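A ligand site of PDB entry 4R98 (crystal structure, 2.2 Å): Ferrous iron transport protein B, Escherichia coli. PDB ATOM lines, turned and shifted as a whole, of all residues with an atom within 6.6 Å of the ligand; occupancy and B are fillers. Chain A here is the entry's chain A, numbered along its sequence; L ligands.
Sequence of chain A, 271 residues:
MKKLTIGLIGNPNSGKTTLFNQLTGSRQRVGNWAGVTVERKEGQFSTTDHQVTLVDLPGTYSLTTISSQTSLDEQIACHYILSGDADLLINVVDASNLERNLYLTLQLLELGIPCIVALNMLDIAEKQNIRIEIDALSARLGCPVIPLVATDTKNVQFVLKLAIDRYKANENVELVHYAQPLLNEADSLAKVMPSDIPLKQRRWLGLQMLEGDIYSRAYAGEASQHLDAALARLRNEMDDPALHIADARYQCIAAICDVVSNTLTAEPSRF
The backbone NH of Thr 17 is in hydrogen-bond range of an oxygen (O2) of the ligand, at 2.7 Å. The side-chain hydroxyl (OG1) of Thr 17 is in hydrogen-bond range of an oxygen (O2) of the ligand (2.5 Å). The backbone NH (N) of Thr 18 sits at hydrogen-bond distance from an oxygen (O4) of the ligand (2.7 Å). OG1 of Thr 18 sits at hydrogen-bond distance from O4 of the ligand (2.9 Å). The backbone NH of Asn 13 sits at hydrogen-bond distance from an oxygen (O1) of the ligand, 2.8 Å away. N of Ala 150 is in hydrogen-bond range of O10 of the ligand, at 3.0 Å. OD1 of Asp 123 sits at hydrogen-bond distance from N4 of the ligand, 3.1 Å away. N of Ser 14 sits at hydrogen-bond distance from O1 of the ligand (3.2 Å). N of Lys 16 is in hydrogen-bond range of O4 of the ligand (3.2 Å). The backbone NH (N) of Gly 15 lies within hydrogen-bond range of an oxygen (O3) of the ligand (3.2 Å). O10 of the ligand sits at hydrogen-bond distance from N of Met 121 (3.4 Å). OD1 of Asn 120 sits close to O10 of the ligand (3.3 Å).
N of Ala 150 sits at hydrogen-bond distance from OD1 of Asn 120, at 2.9 Å. OG of Ser 14 sits at hydrogen-bond distance from O of Asn 11 (2.7 Å). The backbone NH (N) of Met 121 is in hydrogen-bond range of the backbone carbonyl oxygen (O) of Leu 148.
Residues that only touch the ligand: Asn 11, Pro 12, Ile 124, Val 149 and Thr 151. Within 4 Å of the ligand: Asn 11, Pro 12, Asn 13, Ser 14, Gly 15, Lys 16, Thr 17, Thr 18, Asn 120, Met 121, Asp 123, Ile 124, Val 149, Ala 150 and Thr 151. The nearest printed residue that does not touch the ligand is Leu 148 (4.4 Å).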
ATOM      1  N   GLY A  10      11.652 -17.017   6.228  1.00  0.00           N
ATOM      2  CA  GLY A  10      11.253 -15.683   6.669  1.00  0.00           C
ATOM      3  C   GLY A  10      10.829 -15.613   8.126  1.00  0.00           C
ATOM      4  O   GLY A  10      10.714 -16.630   8.802  1.00  0.00           O
ATOM      5  N   ASN A  11      10.600 -14.388   8.596  1.00  0.00           N
ATOM      6  CA  ASN A  11      10.150 -14.148   9.956  1.00  0.00           C
ATOM      7  C   ASN A  11       8.700 -14.595  10.144  1.00  0.00           C
ATOM      8  O   ASN A  11       7.949 -14.649   9.173  1.00  0.00           O
ATOM      9  CB  ASN A  11      10.267 -12.656  10.314  1.00  0.00           C
ATOM     10  CG  ASN A  11      11.712 -12.179  10.478  1.00  0.00           C
ATOM     11  OD1 ASN A  11      11.922 -11.077  10.986  1.00  0.00           O
ATOM     12  ND2 ASN A  11      12.694 -12.976  10.058  1.00  0.00           N
ATOM     13  N   PRO A  12       8.306 -14.912  11.391  1.00  0.00           N
ATOM     14  CA  PRO A  12       6.913 -15.259  11.654  1.00  0.00           C
ATOM     15  C   PRO A  12       5.995 -14.043  11.490  1.00  0.00           C
ATOM     16  O   PRO A  12       6.369 -12.930  11.869  1.00  0.00           O
ATOM     17  CB  PRO A  12       6.930 -15.737  13.105  1.00  0.00           C
ATOM     18  CG  PRO A  12       8.119 -15.088  13.712  1.00  0.00           C
ATOM     19  CD  PRO A  12       9.131 -14.985  12.619  1.00  0.00           C
ATOM     20  N   ASN A  13       4.812 -14.274  10.928  1.00  0.00           N
ATOM     21  CA  ASN A  13       3.836 -13.232  10.626  1.00  0.00           C
ATOM     22  C   ASN A  13       4.376 -12.197   9.629  1.00  0.00           C
ATOM     23  O   ASN A  13       4.311 -10.982   9.872  1.00  0.00           O
ATOM     24  CB  ASN A  13       3.359 -12.556  11.932  1.00  0.00           C
ATOM     25  CG  ASN A  13       2.021 -11.849  11.777  1.00  0.00           C
ATOM     26  OD1 ASN A  13       1.899 -10.657  12.055  1.00  0.00           O
ATOM     27  ND2 ASN A  13       1.009 -12.585  11.331  1.00  0.00           N
ATOM     28  N   SER A  14       4.903 -12.692   8.518  1.00  0.00           N
ATOM     29  CA  SER A  14       5.392 -11.833   7.426  1.00  0.00           C
ATOM     30  C   SER A  14       4.784 -12.236   6.083  1.00  0.00           C
ATOM     31  O   SER A  14       5.347 -11.964   5.024  1.00  0.00           O
ATOM     32  CB  SER A  14       6.920 -11.888   7.361  1.00  0.00           C
ATOM     33  OG  SER A  14       7.374 -13.181   6.991  1.00  0.00           O
ATOM     34  N   GLY A  15       3.619 -12.894   6.125  1.00  0.00           N
ATOM     35  CA  GLY A  15       2.922 -13.335   4.925  1.00  0.00           C
ATOM     36  C   GLY A  15       3.562 -14.524   4.237  1.00  0.00           C
ATOM     37  O   GLY A  15       3.480 -14.644   3.008  1.00  0.00           O
ATOM     38  N   LYS A  16       4.176 -15.408   5.011  1.00  0.00           N
ATOM     39  CA  LYS A  16       4.888 -16.555   4.464  1.00  0.00           C
ATOM     40  C   LYS A  16       3.930 -17.670   4.012  1.00  0.00           C
ATOM     41  O   LYS A  16       4.074 -18.197   2.906  1.00  0.00           O
ATOM     42  CB  LYS A  16       5.880 -17.108   5.488  1.00  0.00           C
ATOM     43  CG  LYS A  16       6.872 -18.064   4.862  1.00  0.00           C
ATOM     44  CD  LYS A  16       7.710 -18.792   5.896  1.00  0.00           C
ATOM     45  CE  LYS A  16       8.599 -19.828   5.218  1.00  0.00           C
ATOM     46  NZ  LYS A  16       7.795 -20.832   4.467  1.00  0.00           N
ATOM     47  N   THR A  17       2.985 -18.029   4.878  1.00  0.00           N
ATOM     48  CA  THR A  17       2.002 -19.071   4.562  1.00  0.00           C
ATOM     49  C   THR A  17       1.080 -18.638   3.423  1.00  0.00           C
ATOM     50  O   THR A  17       0.668 -19.470   2.606  1.00  0.00           O
ATOM     51  CB  THR A  17       1.155 -19.446   5.801  1.00  0.00           C
ATOM     52  OG1 THR A  17       2.010 -19.777   6.894  1.00  0.00           O
ATOM     53  CG2 THR A  17       0.249 -20.642   5.490  1.00  0.00           C
ATOM     54  N   THR A  18       0.755 -17.350   3.386  1.00  0.00           N
ATOM     55  CA  THR A  18      -0.047 -16.791   2.299  1.00  0.00           C
ATOM     56  C   THR A  18       0.654 -16.991   0.946  1.00  0.00           C
ATOM     57  O   THR A  18       0.042 -17.491   0.001  1.00  0.00           O
ATOM     58  CB  THR A  18      -0.316 -15.285   2.516  1.00  0.00           C
ATOM     59  OG1 THR A  18      -0.914 -15.095   3.806  1.00  0.00           O
ATOM     60  CG2 THR A  18      -1.243 -14.729   1.449  1.00  0.00           C
ATOM     61  N   LEU A  19       1.932 -16.604   0.877  1.00  0.00           N
ATOM     62  CA  LEU A  19       2.702 -16.748  -0.351  1.00  0.00           C
ATOM     63  C   LEU A  19       2.905 -18.211  -0.728  1.00  0.00           C
ATOM     64  O   LEU A  19       2.811 -18.574  -1.907  1.00  0.00           O
ATOM     65  CB  LEU A  19       4.069 -16.056  -0.211  1.00  0.00           C
ATOM     66  CG  LEU A  19       4.934 -16.004  -1.483  1.00  0.00           C
ATOM     67  CD1 LEU A  19       4.280 -15.138  -2.547  1.00  0.00           C
ATOM     68  CD2 LEU A  19       6.326 -15.490  -1.149  1.00  0.00           C
ATOM     69  N   GLY A  59       9.245 -20.689  10.555  1.00  0.00           N
ATOM     70  CA  GLY A  59       9.495 -19.253  10.684  1.00  0.00           C
ATOM     71  C   GLY A  59      10.473 -18.938  11.794  1.00  0.00           C
ATOM     72  O   GLY A  59      10.349 -19.455  12.907  1.00  0.00           O
ATOM     73  N   ASN A 120       7.409  -8.441   0.616  1.00  0.00           N
ATOM     74  CA  ASN A 120       5.965  -8.609   0.757  1.00  0.00           C
ATOM     75  C   ASN A 120       5.349  -7.573   1.705  1.00  0.00           C
ATOM     76  O   ASN A 120       6.072  -6.839   2.383  1.00  0.00           O
ATOM     77  CB  ASN A 120       5.683 -10.024   1.280  1.00  0.00           C
ATOM     78  CG  ASN A 120       4.265 -10.489   0.995  1.00  0.00           C
ATOM     79  OD1 ASN A 120       3.710 -10.205  -0.064  1.00  0.00           O
ATOM     80  ND2 ASN A 120       3.684 -11.218   1.937  1.00  0.00           N
ATOM     81  N   MET A 121       4.016  -7.510   1.721  1.00  0.00           N
ATOM     82  CA  MET A 121       3.270  -6.588   2.587  1.00  0.00           C
ATOM     83  C   MET A 121       3.611  -5.121   2.294  1.00  0.00           C
ATOM     84  O   MET A 121       3.706  -4.306   3.211  1.00  0.00           O
ATOM     85  CB  MET A 121       3.476  -6.922   4.066  1.00  0.00           C
ATOM     86  CG  MET A 121       2.824  -8.222   4.516  1.00  0.00           C
ATOM     87  SD  MET A 121       3.329  -8.699   6.187  1.00  0.00           S
ATOM     88  CE  MET A 121       1.868  -9.565   6.759  1.00  0.00           C
ATOM     89  N   LEU A 122       3.802  -4.805   1.021  1.00  0.00           N
ATOM     90  CA  LEU A 122       4.152  -3.444   0.597  1.00  0.00           C
ATOM     91  C   LEU A 122       2.984  -2.475   0.758  1.00  0.00           C
ATOM     92  O   LEU A 122       3.184  -1.286   1.038  1.00  0.00           O
ATOM     93  CB  LEU A 122       4.650  -3.411  -0.848  1.00  0.00           C
ATOM     94  CG  LEU A 122       6.170  -3.471  -1.048  1.00  0.00           C
ATOM     95  CD1 LEU A 122       6.508  -3.701  -2.512  1.00  0.00           C
ATOM     96  CD2 LEU A 122       6.833  -2.206  -0.544  1.00  0.00           C
ATOM     97  N   ASP A 123       1.754  -2.973   0.581  1.00  0.00           N
ATOM     98  CA  ASP A 123       0.556  -2.162   0.791  1.00  0.00           C
ATOM     99  C   ASP A 123       0.428  -1.669   2.237  1.00  0.00           C
ATOM    100  O   ASP A 123      -0.036  -0.558   2.474  1.00  0.00           O
ATOM    101  CB  ASP A 123      -0.704  -2.926   0.366  1.00  0.00           C
ATOM    102  CG  ASP A 123      -0.888  -4.248   1.110  1.00  0.00           C
ATOM    103  OD1 ASP A 123       0.077  -4.711   1.750  1.00  0.00           O
ATOM    104  OD2 ASP A 123      -1.994  -4.818   1.035  1.00  0.00           O
ATOM    105  N   ILE A 124       0.850  -2.503   3.196  1.00  0.00           N
ATOM    106  CA  ILE A 124       0.844  -2.110   4.611  1.00  0.00           C
ATOM    107  C   ILE A 124       1.924  -1.055   4.862  1.00  0.00           C
ATOM    108  O   ILE A 124       1.696  -0.092   5.596  1.00  0.00           O
ATOM    109  CB  ILE A 124       1.066  -3.318   5.542  1.00  0.00           C
ATOM    110  CG1 ILE A 124      -0.079  -4.333   5.395  1.00  0.00           C
ATOM    111  CG2 ILE A 124       1.149  -2.871   6.996  1.00  0.00           C
ATOM    112  CD1 ILE A 124       0.242  -5.723   5.916  1.00  0.00           C
ATOM    113  N   LYS A 127       0.652   2.113   3.483  1.00  0.00           N
ATOM    114  CA  LYS A 127      -0.334   2.653   4.431  1.00  0.00           C
ATOM    115  C   LYS A 127       0.334   3.291   5.653  1.00  0.00           C
ATOM    116  O   LYS A 127      -0.216   4.231   6.243  1.00  0.00           O
ATOM    117  CB  LYS A 127      -1.333   1.578   4.878  1.00  0.00           C
ATOM    118  CG  LYS A 127      -2.440   1.309   3.874  1.00  0.00           C
ATOM    119  CD  LYS A 127      -3.558   0.471   4.465  1.00  0.00           C
ATOM    120  CE  LYS A 127      -3.113  -0.949   4.788  1.00  0.00           C
ATOM    121  NZ  LYS A 127      -4.268  -1.833   5.100  1.00  0.00           N
ATOM    122  N   LEU A 148       5.791  -7.350  -3.637  1.00  0.00           N
ATOM    123  CA  LEU A 148       4.624  -8.223  -3.553  1.00  0.00           C
ATOM    124  C   LEU A 148       3.517  -7.731  -2.625  1.00  0.00           C
ATOM    125  O   LEU A 148       3.765  -7.037  -1.631  1.00  0.00           O
ATOM    126  CB  LEU A 148       5.039  -9.620  -3.084  1.00  0.00           C
ATOM    127  CG  LEU A 148       5.778 -10.518  -4.083  1.00  0.00           C
ATOM    128  CD1 LEU A 148       6.249 -11.780  -3.382  1.00  0.00           C
ATOM    129  CD2 LEU A 148       4.883 -10.875  -5.273  1.00  0.00           C
ATOM    130  N   VAL A 149       2.292  -8.113  -2.973  1.00  0.00           N
ATOM    131  CA  VAL A 149       1.146  -8.106  -2.078  1.00  0.00           C
ATOM    132  C   VAL A 149       0.614  -9.537  -2.156  1.00  0.00           C
ATOM    133  O   VAL A 149      -0.211  -9.855  -3.009  1.00  0.00           O
ATOM    134  CB  VAL A 149       0.069  -7.091  -2.519  1.00  0.00           C
ATOM    135  CG1 VAL A 149      -1.156  -7.181  -1.613  1.00  0.00           C
ATOM    136  CG2 VAL A 149       0.638  -5.678  -2.507  1.00  0.00           C
ATOM    137  N   ALA A 150       1.119 -10.400  -1.272  1.00  0.00           N
ATOM    138  CA  ALA A 150       0.896 -11.846  -1.355  1.00  0.00           C
ATOM    139  C   ALA A 150      -0.586 -12.233  -1.444  1.00  0.00           C
ATOM    140  O   ALA A 150      -0.931 -13.185  -2.134  1.00  0.00           O
ATOM    141  CB  ALA A 150       1.539 -12.561  -0.176  1.00  0.00           C
ATOM    142  N   THR A 151      -1.442 -11.487  -0.749  1.00  0.00           N
ATOM    143  CA  THR A 151      -2.880 -11.781  -0.725  1.00  0.00           C
ATOM    144  C   THR A 151      -3.572 -11.599  -2.081  1.00  0.00           C
ATOM    145  O   THR A 151      -4.639 -12.181  -2.308  1.00  0.00           O
ATOM    146  CB  THR A 151      -3.599 -10.904   0.324  1.00  0.00           C
ATOM    147  OG1 THR A 151      -3.270  -9.529   0.123  1.00  0.00           O
ATOM    148  CG2 THR A 151      -3.201 -11.329   1.735  1.00  0.00           C
ATOM    149  N   ASP A 152      -2.974 -10.793  -2.966  1.00  0.00           N
ATOM    150  CA  ASP A 152      -3.531 -10.551  -4.294  1.00  0.00           C
ATOM    151  C   ASP A 152      -2.918 -11.498  -5.326  1.00  0.00           C
ATOM    152  O   ASP A 152      -1.719 -11.415  -5.625  1.00  0.00           O
ATOM    153  CB  ASP A 152      -3.265  -9.091  -4.703  1.00  0.00           C
ATOM    154  CG  ASP A 152      -3.987  -8.694  -5.986  1.00  0.00           C
ATOM    155  OD1 ASP A 152      -5.034  -9.292  -6.303  1.00  0.00           O
ATOM    156  OD2 ASP A 152      -3.503  -7.762  -6.663  1.00  0.00           O
HETATM  157  N1  LIG L   1       2.469 -16.828  10.087  1.00  0.00           N
HETATM  158  P1  LIG L   1       3.095 -16.359   8.517  1.00  0.00           P
HETATM  159  O1  LIG L   1       4.479 -15.855   8.670  1.00  0.00           O
HETATM  160  O2  LIG L   1       3.101 -17.627   7.550  1.00  0.00           O
HETATM  161  O3  LIG L   1       2.177 -15.197   7.892  1.00  0.00           O
HETATM  162  P2  LIG L   1       0.779 -15.549   7.152  1.00  0.00           P
HETATM  163  O4  LIG L   1       1.080 -15.957   5.728  1.00  0.00           O
HETATM  164  O5  LIG L   1      -0.005 -16.478   8.050  1.00  0.00           O
HETATM  165  O6  LIG L   1       0.036 -14.128   7.127  1.00  0.00           O
HETATM  166  C1  LIG L   1      -0.226 -13.429   8.349  1.00  0.00           C
HETATM  167  C2  LIG L   1      -1.340 -12.407   8.146  1.00  0.00           C
HETATM  168  O7  LIG L   1      -0.899 -11.359   7.279  1.00  0.00           O
HETATM  169  C3  LIG L   1      -2.581 -13.016   7.514  1.00  0.00           C
HETATM  170  O8  LIG L   1      -3.743 -12.555   8.200  1.00  0.00           O
HETATM  171  C4  LIG L   1      -2.563 -12.533   6.072  1.00  0.00           C
HETATM  172  O9  LIG L   1      -3.874 -12.310   5.554  1.00  0.00           O
HETATM  173  C5  LIG L   1      -1.758 -11.239   6.142  1.00  0.00           C
HETATM  174  N2  LIG L   1      -0.948 -10.981   4.924  1.00  0.00           N
HETATM  175  C6  LIG L   1      -0.090 -11.820   4.322  1.00  0.00           C
HETATM  176  N3  LIG L   1       0.485 -11.239   3.240  1.00  0.00           N
HETATM  177  C7  LIG L   1      -0.005  -9.978   3.151  1.00  0.00           C
HETATM  178  C8  LIG L   1       0.167  -8.820   2.248  1.00  0.00           C
HETATM  179  O10 LIG L   1       0.945  -8.868   1.270  1.00  0.00           O
HETATM  180  N4  LIG L   1      -0.537  -7.701   2.511  1.00  0.00           N
HETATM  181  C9  LIG L   1      -1.388  -7.613   3.558  1.00  0.00           C
HETATM  182  N5  LIG L   1      -2.075  -6.465   3.771  1.00  0.00           N
HETATM  183  N6  LIG L   1      -1.591  -8.647   4.420  1.00  0.00           N
HETATM  184  C10 LIG L   1      -0.943  -9.821   4.266  1.00  0.00           C
